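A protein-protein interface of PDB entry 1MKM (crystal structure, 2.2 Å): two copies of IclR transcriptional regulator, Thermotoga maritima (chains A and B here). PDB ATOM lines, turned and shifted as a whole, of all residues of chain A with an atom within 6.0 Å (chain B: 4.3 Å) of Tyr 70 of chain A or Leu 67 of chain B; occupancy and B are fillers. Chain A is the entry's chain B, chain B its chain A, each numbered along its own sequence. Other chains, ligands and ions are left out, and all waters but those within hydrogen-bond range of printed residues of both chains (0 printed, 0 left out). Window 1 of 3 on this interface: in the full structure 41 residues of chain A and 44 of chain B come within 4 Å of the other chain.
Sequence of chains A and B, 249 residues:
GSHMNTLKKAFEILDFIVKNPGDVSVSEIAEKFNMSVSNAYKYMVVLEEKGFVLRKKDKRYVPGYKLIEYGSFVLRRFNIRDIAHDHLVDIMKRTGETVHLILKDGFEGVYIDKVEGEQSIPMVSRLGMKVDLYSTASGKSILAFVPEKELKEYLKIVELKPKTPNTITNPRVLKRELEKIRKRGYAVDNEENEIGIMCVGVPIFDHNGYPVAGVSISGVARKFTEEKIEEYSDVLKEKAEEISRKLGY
Of chain B, only Leu 14 (3.4 Å), Asp 15 (2.4 Å), Val 18 (3.7 Å) and Leu 67 (3.7 Å) come within 4 Å of Tyr 70 of chain A. Of the printed residues of chain B, Gly 71 of chain A touches Leu 67 and Ile 68. Of the printed residues of chain B, Phe 73 of chain A touches Val 18 (3.6 Å). Printed residues of chain B within 4 Å of Leu 75 of chain A: Ile 68 (3.7 Å). Phe 52 of chain B touches none of the printed residues of chain A. Printed residues of chain A within 4 Å of Pro 63 of chain B: Val 74 (3.8 Å). Of the printed residues of chain A, Leu 67 of chain B touches Leu 67, Tyr 70, Gly 71 and Val 74. Of the printed residues of chain A, Tyr 70 of chain B touches Leu 67. The nearest printed residue of chain B that does not touch Tyr 70 of chain A is Ile 68 of chain B (5.6 Å). The nearest printed residue of chain A that does not touch Leu 14 of chain B is Phe 52 of chain A (4.4 Å).
Among the printed residues, pairs that only touch across the chains: Leu 67 of chain A with Leu 67 of chain B (3.97 Å), Leu 67 of chain A with Tyr 70 of chain B (3.8 Å), Leu 67 of chain A with Gly 71 of chain B (3.5 Å), Ile 68 of chain A with Gly 71 of chain B (3.9 Å), Tyr 70 of chain A with Leu 14 of chain B (3.4 Å), Tyr 70 of chain A with Val 18 of chain B (3.7 Å), Tyr 70 of chain A with Leu 67 of chain B (3.7 Å), Gly 71 of chain A with Leu 67 of chain B (3.4 Å), Gly 71 of chain A with Ile 68 of chain B (3.9 Å), Phe 73 of chain A with Val 18 of chain B (3.6 Å), Val 74 of chain A with Pro 63 of chain B (3.8 Å), Val 74 of chain A with Leu 67 of chain B (3.96 Å), Val 74 of chain A with Ile 68 of chain B (3.7 Å) and Leu 75 of chain A with Ile 68 of chain B (3.7 Å).
OH of Tyr 70 of chain B sits at hydrogen-bond distance from NZ of Lys 66 of chain B (2.8 Å). The backbone carbonyl oxygen (O) of Ile 68 of chain A lies within hydrogen-bond range of the side-chain hydroxyl (OG) of Ser 72 of chain A, at 3.3 Å.
The side-chain carboxylate (OD1) of Asp 15 of chain B lies within hydrogen-bond range of the side-chain hydroxyl (OH) of Tyr 70 of chain A, 2.4 Å away.
Leu 67 of chain B touches its own counterpart, Leu 67 of chain A. Leu 67 of chain A touches Tyr 70 of chain B, and with the chains exchanged Tyr 70 of chain A touches Leu 67 of chain B. Leu 67 of chain A touches Gly 71 of chain B, and with the chains exchanged Gly 71 of chain A touches Leu 67 of chain B. Ile 68 of chain A touches Gly 71 of chain B, and with the chains exchanged Gly 71 of chain A touches Ile 68 of chain B. 8 positions are printed for both chains.
Of the 12 printed residues of chain A, 7 touch a printed residue of chain B. Hydrophobic or aromatic side chains of chain B that line the printed part of chain A: Leu 14, Val 18, Pro 63, Leu 67, Ile 68 and Tyr 70.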
ATOM      1  N   PHE A  52      15.582  36.608  -7.039  1.00  0.00           N
ATOM      2  CA  PHE A  52      14.159  36.885  -6.854  1.00  0.00           C
ATOM      3  C   PHE A  52      13.743  38.080  -7.668  1.00  0.00           C
ATOM      4  O   PHE A  52      12.572  38.253  -8.004  1.00  0.00           O
ATOM      5  CB  PHE A  52      13.847  37.137  -5.375  1.00  0.00           C
ATOM      6  CG  PHE A  52      13.911  35.894  -4.541  1.00  0.00           C
ATOM      7  CD1 PHE A  52      15.116  35.476  -3.976  1.00  0.00           C
ATOM      8  CD2 PHE A  52      12.794  35.088  -4.399  1.00  0.00           C
ATOM      9  CE1 PHE A  52      15.202  34.257  -3.283  1.00  0.00           C
ATOM     10  CE2 PHE A  52      12.875  33.878  -3.714  1.00  0.00           C
ATOM     11  CZ  PHE A  52      14.081  33.461  -3.157  1.00  0.00           C
ATOM     12  N   TYR A  65      13.675  34.902 -11.938  1.00  0.00           N
ATOM     13  CA  TYR A  65      13.254  33.555 -12.282  1.00  0.00           C
ATOM     14  C   TYR A  65      13.164  32.625 -11.085  1.00  0.00           C
ATOM     15  O   TYR A  65      12.488  31.605 -11.147  1.00  0.00           O
ATOM     16  CB  TYR A  65      14.258  32.960 -13.264  1.00  0.00           C
ATOM     17  CG  TYR A  65      15.466  32.395 -12.553  1.00  0.00           C
ATOM     18  CD1 TYR A  65      15.492  31.058 -12.140  1.00  0.00           C
ATOM     19  CD2 TYR A  65      16.535  33.215 -12.193  1.00  0.00           C
ATOM     20  CE1 TYR A  65      16.538  30.557 -11.387  1.00  0.00           C
ATOM     21  CE2 TYR A  65      17.597  32.718 -11.426  1.00  0.00           C
ATOM     22  CZ  TYR A  65      17.586  31.390 -11.030  1.00  0.00           C
ATOM     23  OH  TYR A  65      18.613  30.886 -10.265  1.00  0.00           O
ATOM     24  N   LYS A  66      13.882  32.947 -10.011  1.00  0.00           N
ATOM     25  CA  LYS A  66      13.900  32.090  -8.827  1.00  0.00           C
ATOM     26  C   LYS A  66      12.522  31.574  -8.426  1.00  0.00           C
ATOM     27  O   LYS A  66      12.299  30.368  -8.352  1.00  0.00           O
ATOM     28  CB  LYS A  66      14.543  32.829  -7.650  1.00  0.00           C
ATOM     29  CG  LYS A  66      14.703  31.995  -6.420  1.00  0.00           C
ATOM     30  CD  LYS A  66      15.483  30.727  -6.724  1.00  0.00           C
ATOM     31  CE  LYS A  66      16.898  31.013  -7.215  1.00  0.00           C
ATOM     32  NZ  LYS A  66      17.641  29.736  -7.456  1.00  0.00           N
ATOM     33  N   LEU A  67      11.605  32.494  -8.166  1.00  0.00           N
ATOM     34  CA  LEU A  67      10.245  32.150  -7.770  1.00  0.00           C
ATOM     35  C   LEU A  67       9.627  31.129  -8.746  1.00  0.00           C
ATOM     36  O   LEU A  67       8.963  30.171  -8.327  1.00  0.00           O
ATOM     37  CB  LEU A  67       9.434  33.441  -7.688  1.00  0.00           C
ATOM     38  CG  LEU A  67       8.944  33.914  -6.305  1.00  0.00           C
ATOM     39  CD1 LEU A  67       9.922  33.580  -5.225  1.00  0.00           C
ATOM     40  CD2 LEU A  67       8.672  35.396  -6.346  1.00  0.00           C
ATOM     41  N   ILE A  68       9.880  31.321 -10.044  1.00  0.00           N
ATOM     42  CA  ILE A  68       9.392  30.398 -11.064  1.00  0.00           C
ATOM     43  C   ILE A  68       9.979  29.018 -10.780  1.00  0.00           C
ATOM     44  O   ILE A  68       9.268  28.010 -10.763  1.00  0.00           O
ATOM     45  CB  ILE A  68       9.803  30.843 -12.481  1.00  0.00           C
ATOM     46  CG1 ILE A  68       9.187  32.213 -12.794  1.00  0.00           C
ATOM     47  CG2 ILE A  68       9.322  29.829 -13.480  1.00  0.00           C
ATOM     48  CD1 ILE A  68       9.740  32.918 -14.038  1.00  0.00           C
ATOM     49  N   GLU A  69      11.284  28.975 -10.541  1.00  0.00           N
ATOM     50  CA  GLU A  69      11.936  27.715 -10.218  1.00  0.00           C
ATOM     51  C   GLU A  69      11.348  27.097  -8.934  1.00  0.00           C
ATOM     52  O   GLU A  69      11.160  25.878  -8.842  1.00  0.00           O
ATOM     53  CB  GLU A  69      13.438  27.943 -10.010  1.00  0.00           C
ATOM     54  CG  GLU A  69      14.198  26.676  -9.666  1.00  0.00           C
ATOM     55  CD  GLU A  69      15.627  26.928  -9.195  1.00  0.00           C
ATOM     56  OE1 GLU A  69      16.077  28.096  -9.181  1.00  0.00           O
ATOM     57  OE2 GLU A  69      16.298  25.941  -8.833  1.00  0.00           O
ATOM     58  N   TYR A  70      11.066  27.933  -7.935  1.00  0.00           N
ATOM     59  CA  TYR A  70      10.534  27.432  -6.664  1.00  0.00           C
ATOM     60  C   TYR A  70       9.166  26.784  -6.835  1.00  0.00           C
ATOM     61  O   TYR A  70       8.898  25.717  -6.282  1.00  0.00           O
ATOM     62  CB  TYR A  70      10.461  28.562  -5.629  1.00  0.00           C
ATOM     63  CG  TYR A  70      11.774  28.831  -4.929  1.00  0.00           C
ATOM     64  CD1 TYR A  70      12.923  28.101  -5.251  1.00  0.00           C
ATOM     65  CD2 TYR A  70      11.874  29.821  -3.934  1.00  0.00           C
ATOM     66  CE1 TYR A  70      14.131  28.347  -4.606  1.00  0.00           C
ATOM     67  CE2 TYR A  70      13.075  30.078  -3.289  1.00  0.00           C
ATOM     68  CZ  TYR A  70      14.196  29.339  -3.627  1.00  0.00           C
ATOM     69  OH  TYR A  70      15.383  29.576  -3.000  1.00  0.00           O
ATOM     70  N   GLY A  71       8.307  27.444  -7.598  1.00  0.00           N
ATOM     71  CA  GLY A  71       6.987  26.908  -7.846  1.00  0.00           C
ATOM     72  C   GLY A  71       7.060  25.522  -8.470  1.00  0.00           C
ATOM     73  O   GLY A  71       6.334  24.622  -8.047  1.00  0.00           O
ATOM     74  N   SER A  72       7.935  25.353  -9.467  1.00  0.00           N
ATOM     75  CA  SER A  72       8.109  24.061 -10.148  1.00  0.00           C
ATOM     76  C   SER A  72       8.562  22.980  -9.185  1.00  0.00           C
ATOM     77  O   SER A  72       8.104  21.844  -9.270  1.00  0.00           O
ATOM     78  CB  SER A  72       9.134  24.176 -11.275  1.00  0.00           C
ATOM     79  OG  SER A  72       8.725  25.144 -12.204  1.00  0.00           O
ATOM     80  N   PHE A  73       9.479  23.335  -8.280  1.00  0.00           N
ATOM     81  CA  PHE A  73       9.985  22.404  -7.268  1.00  0.00           C
ATOM     82  C   PHE A  73       8.852  21.897  -6.369  1.00  0.00           C
ATOM     83  O   PHE A  73       8.801  20.716  -6.017  1.00  0.00           O
ATOM     84  CB  PHE A  73      11.035  23.090  -6.383  1.00  0.00           C
ATOM     85  CG  PHE A  73      12.457  22.881  -6.827  1.00  0.00           C
ATOM     86  CD1 PHE A  73      13.192  23.928  -7.370  1.00  0.00           C
ATOM     87  CD2 PHE A  73      13.079  21.645  -6.660  1.00  0.00           C
ATOM     88  CE1 PHE A  73      14.538  23.754  -7.736  1.00  0.00           C
ATOM     89  CE2 PHE A  73      14.422  21.455  -7.022  1.00  0.00           C
ATOM     90  CZ  PHE A  73      15.151  22.516  -7.561  1.00  0.00           C
ATOM     91  N   VAL A  74       7.953  22.795  -5.978  1.00  0.00           N
ATOM     92  CA  VAL A  74       6.844  22.402  -5.116  1.00  0.00           C
ATOM     93  C   VAL A  74       5.853  21.561  -5.929  1.00  0.00           C
ATOM     94  O   VAL A  74       5.409  20.524  -5.459  1.00  0.00           O
ATOM     95  CB  VAL A  74       6.111  23.624  -4.524  1.00  0.00           C
ATOM     96  CG1 VAL A  74       5.022  23.160  -3.585  1.00  0.00           C
ATOM     97  CG2 VAL A  74       7.096  24.525  -3.777  1.00  0.00           C
ATOM     98  N   LEU A  75       5.512  22.008  -7.140  1.00  0.00           N
ATOM     99  CA  LEU A  75       4.595  21.240  -8.001  1.00  0.00           C
ATOM    100  C   LEU A  75       5.210  19.870  -8.253  1.00  0.00           C
ATOM    101  O   LEU A  75       4.524  18.859  -8.338  1.00  0.00           O
ATOM    102  CB  LEU A  75       4.382  21.963  -9.336  1.00  0.00           C
ATOM    103  CG  LEU A  75       3.390  23.127  -9.307  1.00  0.00           C
ATOM    104  CD1 LEU A  75       3.556  24.002 -10.512  1.00  0.00           C
ATOM    105  CD2 LEU A  75       1.988  22.575  -9.225  1.00  0.00           C
ATOM    106  N   LEU B  14      15.033  29.063   3.263  1.00  0.00           N
ATOM    107  CA  LEU B  14      13.910  28.867   2.361  1.00  0.00           C
ATOM    108  C   LEU B  14      14.375  27.978   1.210  1.00  0.00           C
ATOM    109  O   LEU B  14      13.665  27.060   0.800  1.00  0.00           O
ATOM    110  CB  LEU B  14      13.402  30.219   1.831  1.00  0.00           C
ATOM    111  CG  LEU B  14      11.979  30.334   1.251  1.00  0.00           C
ATOM    112  CD1 LEU B  14      12.014  30.932  -0.154  1.00  0.00           C
ATOM    113  CD2 LEU B  14      11.321  28.998   1.223  1.00  0.00           C
ATOM    114  N   ASP B  15      15.575  28.249   0.699  1.00  0.00           N
ATOM    115  CA  ASP B  15      16.133  27.481  -0.406  1.00  0.00           C
ATOM    116  C   ASP B  15      16.284  26.022  -0.019  1.00  0.00           C
ATOM    117  O   ASP B  15      15.949  25.126  -0.786  1.00  0.00           O
ATOM    118  CB  ASP B  15      17.499  28.041  -0.836  1.00  0.00           C
ATOM    119  CG  ASP B  15      17.905  27.585  -2.239  1.00  0.00           C
ATOM    120  OD1 ASP B  15      17.234  27.994  -3.216  1.00  0.00           O
ATOM    121  OD2 ASP B  15      18.886  26.817  -2.363  1.00  0.00           O
ATOM    122  N   VAL B  18      12.699  24.271   0.040  1.00  0.00           N
ATOM    123  CA  VAL B  18      12.142  24.086  -1.279  1.00  0.00           C
ATOM    124  C   VAL B  18      12.852  22.970  -2.048  1.00  0.00           C
ATOM    125  O   VAL B  18      12.210  22.204  -2.775  1.00  0.00           O
ATOM    126  CB  VAL B  18      12.221  25.391  -2.115  1.00  0.00           C
ATOM    127  CG1 VAL B  18      11.651  25.145  -3.511  1.00  0.00           C
ATOM    128  CG2 VAL B  18      11.461  26.510  -1.432  1.00  0.00           C
ATOM    129  N   PHE B  52       5.118  30.714   2.650  1.00  0.00           N
ATOM    130  CA  PHE B  52       6.181  30.109   1.862  1.00  0.00           C
ATOM    131  C   PHE B  52       6.547  28.776   2.450  1.00  0.00           C
ATOM    132  O   PHE B  52       7.363  28.051   1.888  1.00  0.00           O
ATOM    133  CB  PHE B  52       7.442  30.976   1.860  1.00  0.00           C
ATOM    134  CG  PHE B  52       7.280  32.309   1.175  1.00  0.00           C
ATOM    135  CD1 PHE B  52       6.415  33.272   1.677  1.00  0.00           C
ATOM    136  CD2 PHE B  52       8.039  32.620   0.060  1.00  0.00           C
ATOM    137  CE1 PHE B  52       6.319  34.529   1.076  1.00  0.00           C
ATOM    138  CE2 PHE B  52       7.945  33.869  -0.541  1.00  0.00           C
ATOM    139  CZ  PHE B  52       7.083  34.822  -0.028  1.00  0.00           C
ATOM    140  N   PRO B  63       7.669  22.791   1.934  1.00  0.00           N
ATOM    141  CA  PRO B  63       7.366  24.048   1.228  1.00  0.00           C
ATOM    142  C   PRO B  63       5.870  24.351   1.076  1.00  0.00           C
ATOM    143  O   PRO B  63       5.044  23.434   0.981  1.00  0.00           O
ATOM    144  CB  PRO B  63       8.089  23.890  -0.116  1.00  0.00           C
ATOM    145  CG  PRO B  63       8.313  22.420  -0.259  1.00  0.00           C
ATOM    146  CD  PRO B  63       8.537  21.913   1.128  1.00  0.00           C
ATOM    147  N   GLY B  64       5.551  25.650   1.072  1.00  0.00           N
ATOM    148  CA  GLY B  64       4.182  26.136   0.957  1.00  0.00           C
ATOM    149  C   GLY B  64       3.613  26.406  -0.440  1.00  0.00           C
ATOM    150  O   GLY B  64       4.338  26.570  -1.420  1.00  0.00           O
ATOM    151  N   TYR B  65       2.289  26.472  -0.508  1.00  0.00           N
ATOM    152  CA  TYR B  65       1.573  26.679  -1.749  1.00  0.00           C
ATOM    153  C   TYR B  65       1.813  28.039  -2.371  1.00  0.00           C
ATOM    154  O   TYR B  65       1.726  28.198  -3.589  1.00  0.00           O
ATOM    155  CB  TYR B  65       0.087  26.437  -1.503  1.00  0.00           C
ATOM    156  CG  TYR B  65      -0.199  25.001  -1.103  1.00  0.00           C
ATOM    157  CD1 TYR B  65      -0.994  24.694   0.002  1.00  0.00           C
ATOM    158  CD2 TYR B  65       0.332  23.945  -1.838  1.00  0.00           C
ATOM    159  CE1 TYR B  65      -1.247  23.375   0.364  1.00  0.00           C
ATOM    160  CE2 TYR B  65       0.082  22.623  -1.486  1.00  0.00           C
ATOM    161  CZ  TYR B  65      -0.704  22.347  -0.385  1.00  0.00           C
ATOM    162  OH  TYR B  65      -0.908  21.029  -0.044  1.00  0.00           O
ATOM    163  N   LYS B  66       2.150  29.016  -1.539  1.00  0.00           N
ATOM    164  CA  LYS B  66       2.410  30.365  -2.020  1.00  0.00           C
ATOM    165  C   LYS B  66       3.528  30.394  -3.064  1.00  0.00           C
ATOM    166  O   LYS B  66       3.498  31.211  -3.963  1.00  0.00           O
ATOM    167  CB  LYS B  66       2.792  31.277  -0.847  1.00  0.00           C
ATOM    168  CG  LYS B  66       2.739  32.757  -1.170  1.00  0.00           C
ATOM    169  CD  LYS B  66       1.309  33.179  -1.477  1.00  0.00           C
ATOM    170  CE  LYS B  66       0.919  34.413  -0.681  1.00  0.00           C
ATOM    171  NZ  LYS B  66       1.906  35.530  -0.852  1.00  0.00           N
ATOM    172  N   LEU B  67       4.522  29.528  -2.927  1.00  0.00           N
ATOM    173  CA  LEU B  67       5.618  29.473  -3.892  1.00  0.00           C
ATOM    174  C   LEU B  67       5.074  29.118  -5.281  1.00  0.00           C
ATOM    175  O   LEU B  67       5.611  29.543  -6.298  1.00  0.00           O
ATOM    176  CB  LEU B  67       6.664  28.446  -3.442  1.00  0.00           C
ATOM    177  CG  LEU B  67       7.394  28.938  -2.206  1.00  0.00           C
ATOM    178  CD1 LEU B  67       8.005  27.768  -1.452  1.00  0.00           C
ATOM    179  CD2 LEU B  67       8.449  29.977  -2.632  1.00  0.00           C
ATOM    180  N   ILE B  68       3.994  28.350  -5.320  1.00  0.00           N
ATOM    181  CA  ILE B  68       3.399  28.002  -6.603  1.00  0.00           C
ATOM    182  C   ILE B  68       2.635  29.222  -7.056  1.00  0.00           C
ATOM    183  O   ILE B  68       2.725  29.633  -8.211  1.00  0.00           O
ATOM    184  CB  ILE B  68       2.433  26.796  -6.498  1.00  0.00           C
ATOM    185  CG1 ILE B  68       3.177  25.578  -5.940  1.00  0.00           C
ATOM    186  CG2 ILE B  68       1.864  26.489  -7.847  1.00  0.00           C
ATOM    187  CD1 ILE B  68       2.381  24.266  -5.943  1.00  0.00           C
ATOM    188  N   GLU B  69       1.902  29.832  -6.135  1.00  0.00           N
ATOM    189  CA  GLU B  69       1.114  31.019  -6.489  1.00  0.00           C
ATOM    190  C   GLU B  69       1.995  32.093  -7.110  1.00  0.00           C
ATOM    191  O   GLU B  69       1.661  32.664  -8.155  1.00  0.00           O
ATOM    192  CB  GLU B  69       0.402  31.554  -5.252  1.00  0.00           C
ATOM    193  CG  GLU B  69      -0.502  32.734  -5.512  1.00  0.00           C
ATOM    194  CD  GLU B  69      -1.701  32.744  -4.587  1.00  0.00           C
ATOM    195  OE1 GLU B  69      -1.515  32.493  -3.378  1.00  0.00           O
ATOM    196  OE2 GLU B  69      -2.827  33.004  -5.067  1.00  0.00           O
ATOM    197  N   TYR B  70       3.128  32.357  -6.462  1.00  0.00           N
ATOM    198  CA  TYR B  70       4.089  33.350  -6.940  1.00  0.00           C
ATOM    199  C   TYR B  70       4.768  32.888  -8.221  1.00  0.00           C
ATOM    200  O   TYR B  70       5.022  33.686  -9.123  1.00  0.00           O
ATOM    201  CB  TYR B  70       5.191  33.585  -5.915  1.00  0.00           C
ATOM    202  CG  TYR B  70       4.829  34.471  -4.766  1.00  0.00           C
ATOM    203  CD1 TYR B  70       3.944  35.530  -4.924  1.00  0.00           C
ATOM    204  CD2 TYR B  70       5.448  34.309  -3.533  1.00  0.00           C
ATOM    205  CE1 TYR B  70       3.691  36.408  -3.883  1.00  0.00           C
ATOM    206  CE2 TYR B  70       5.201  35.181  -2.490  1.00  0.00           C
ATOM    207  CZ  TYR B  70       4.326  36.225  -2.671  1.00  0.00           C
ATOM    208  OH  TYR B  70       4.101  37.083  -1.623  1.00  0.00           O
ATOM    209  N   GLY B  71       5.100  31.596  -8.258  1.00  0.00           N
ATOM    210  CA  GLY B  71       5.776  31.037  -9.411  1.00  0.00           C
ATOM    211  C   GLY B  71       5.008  31.235 -10.698  1.00  0.00           C
ATOM    212  O   GLY B  71       5.512  31.795 -11.663  1.00  0.00           O
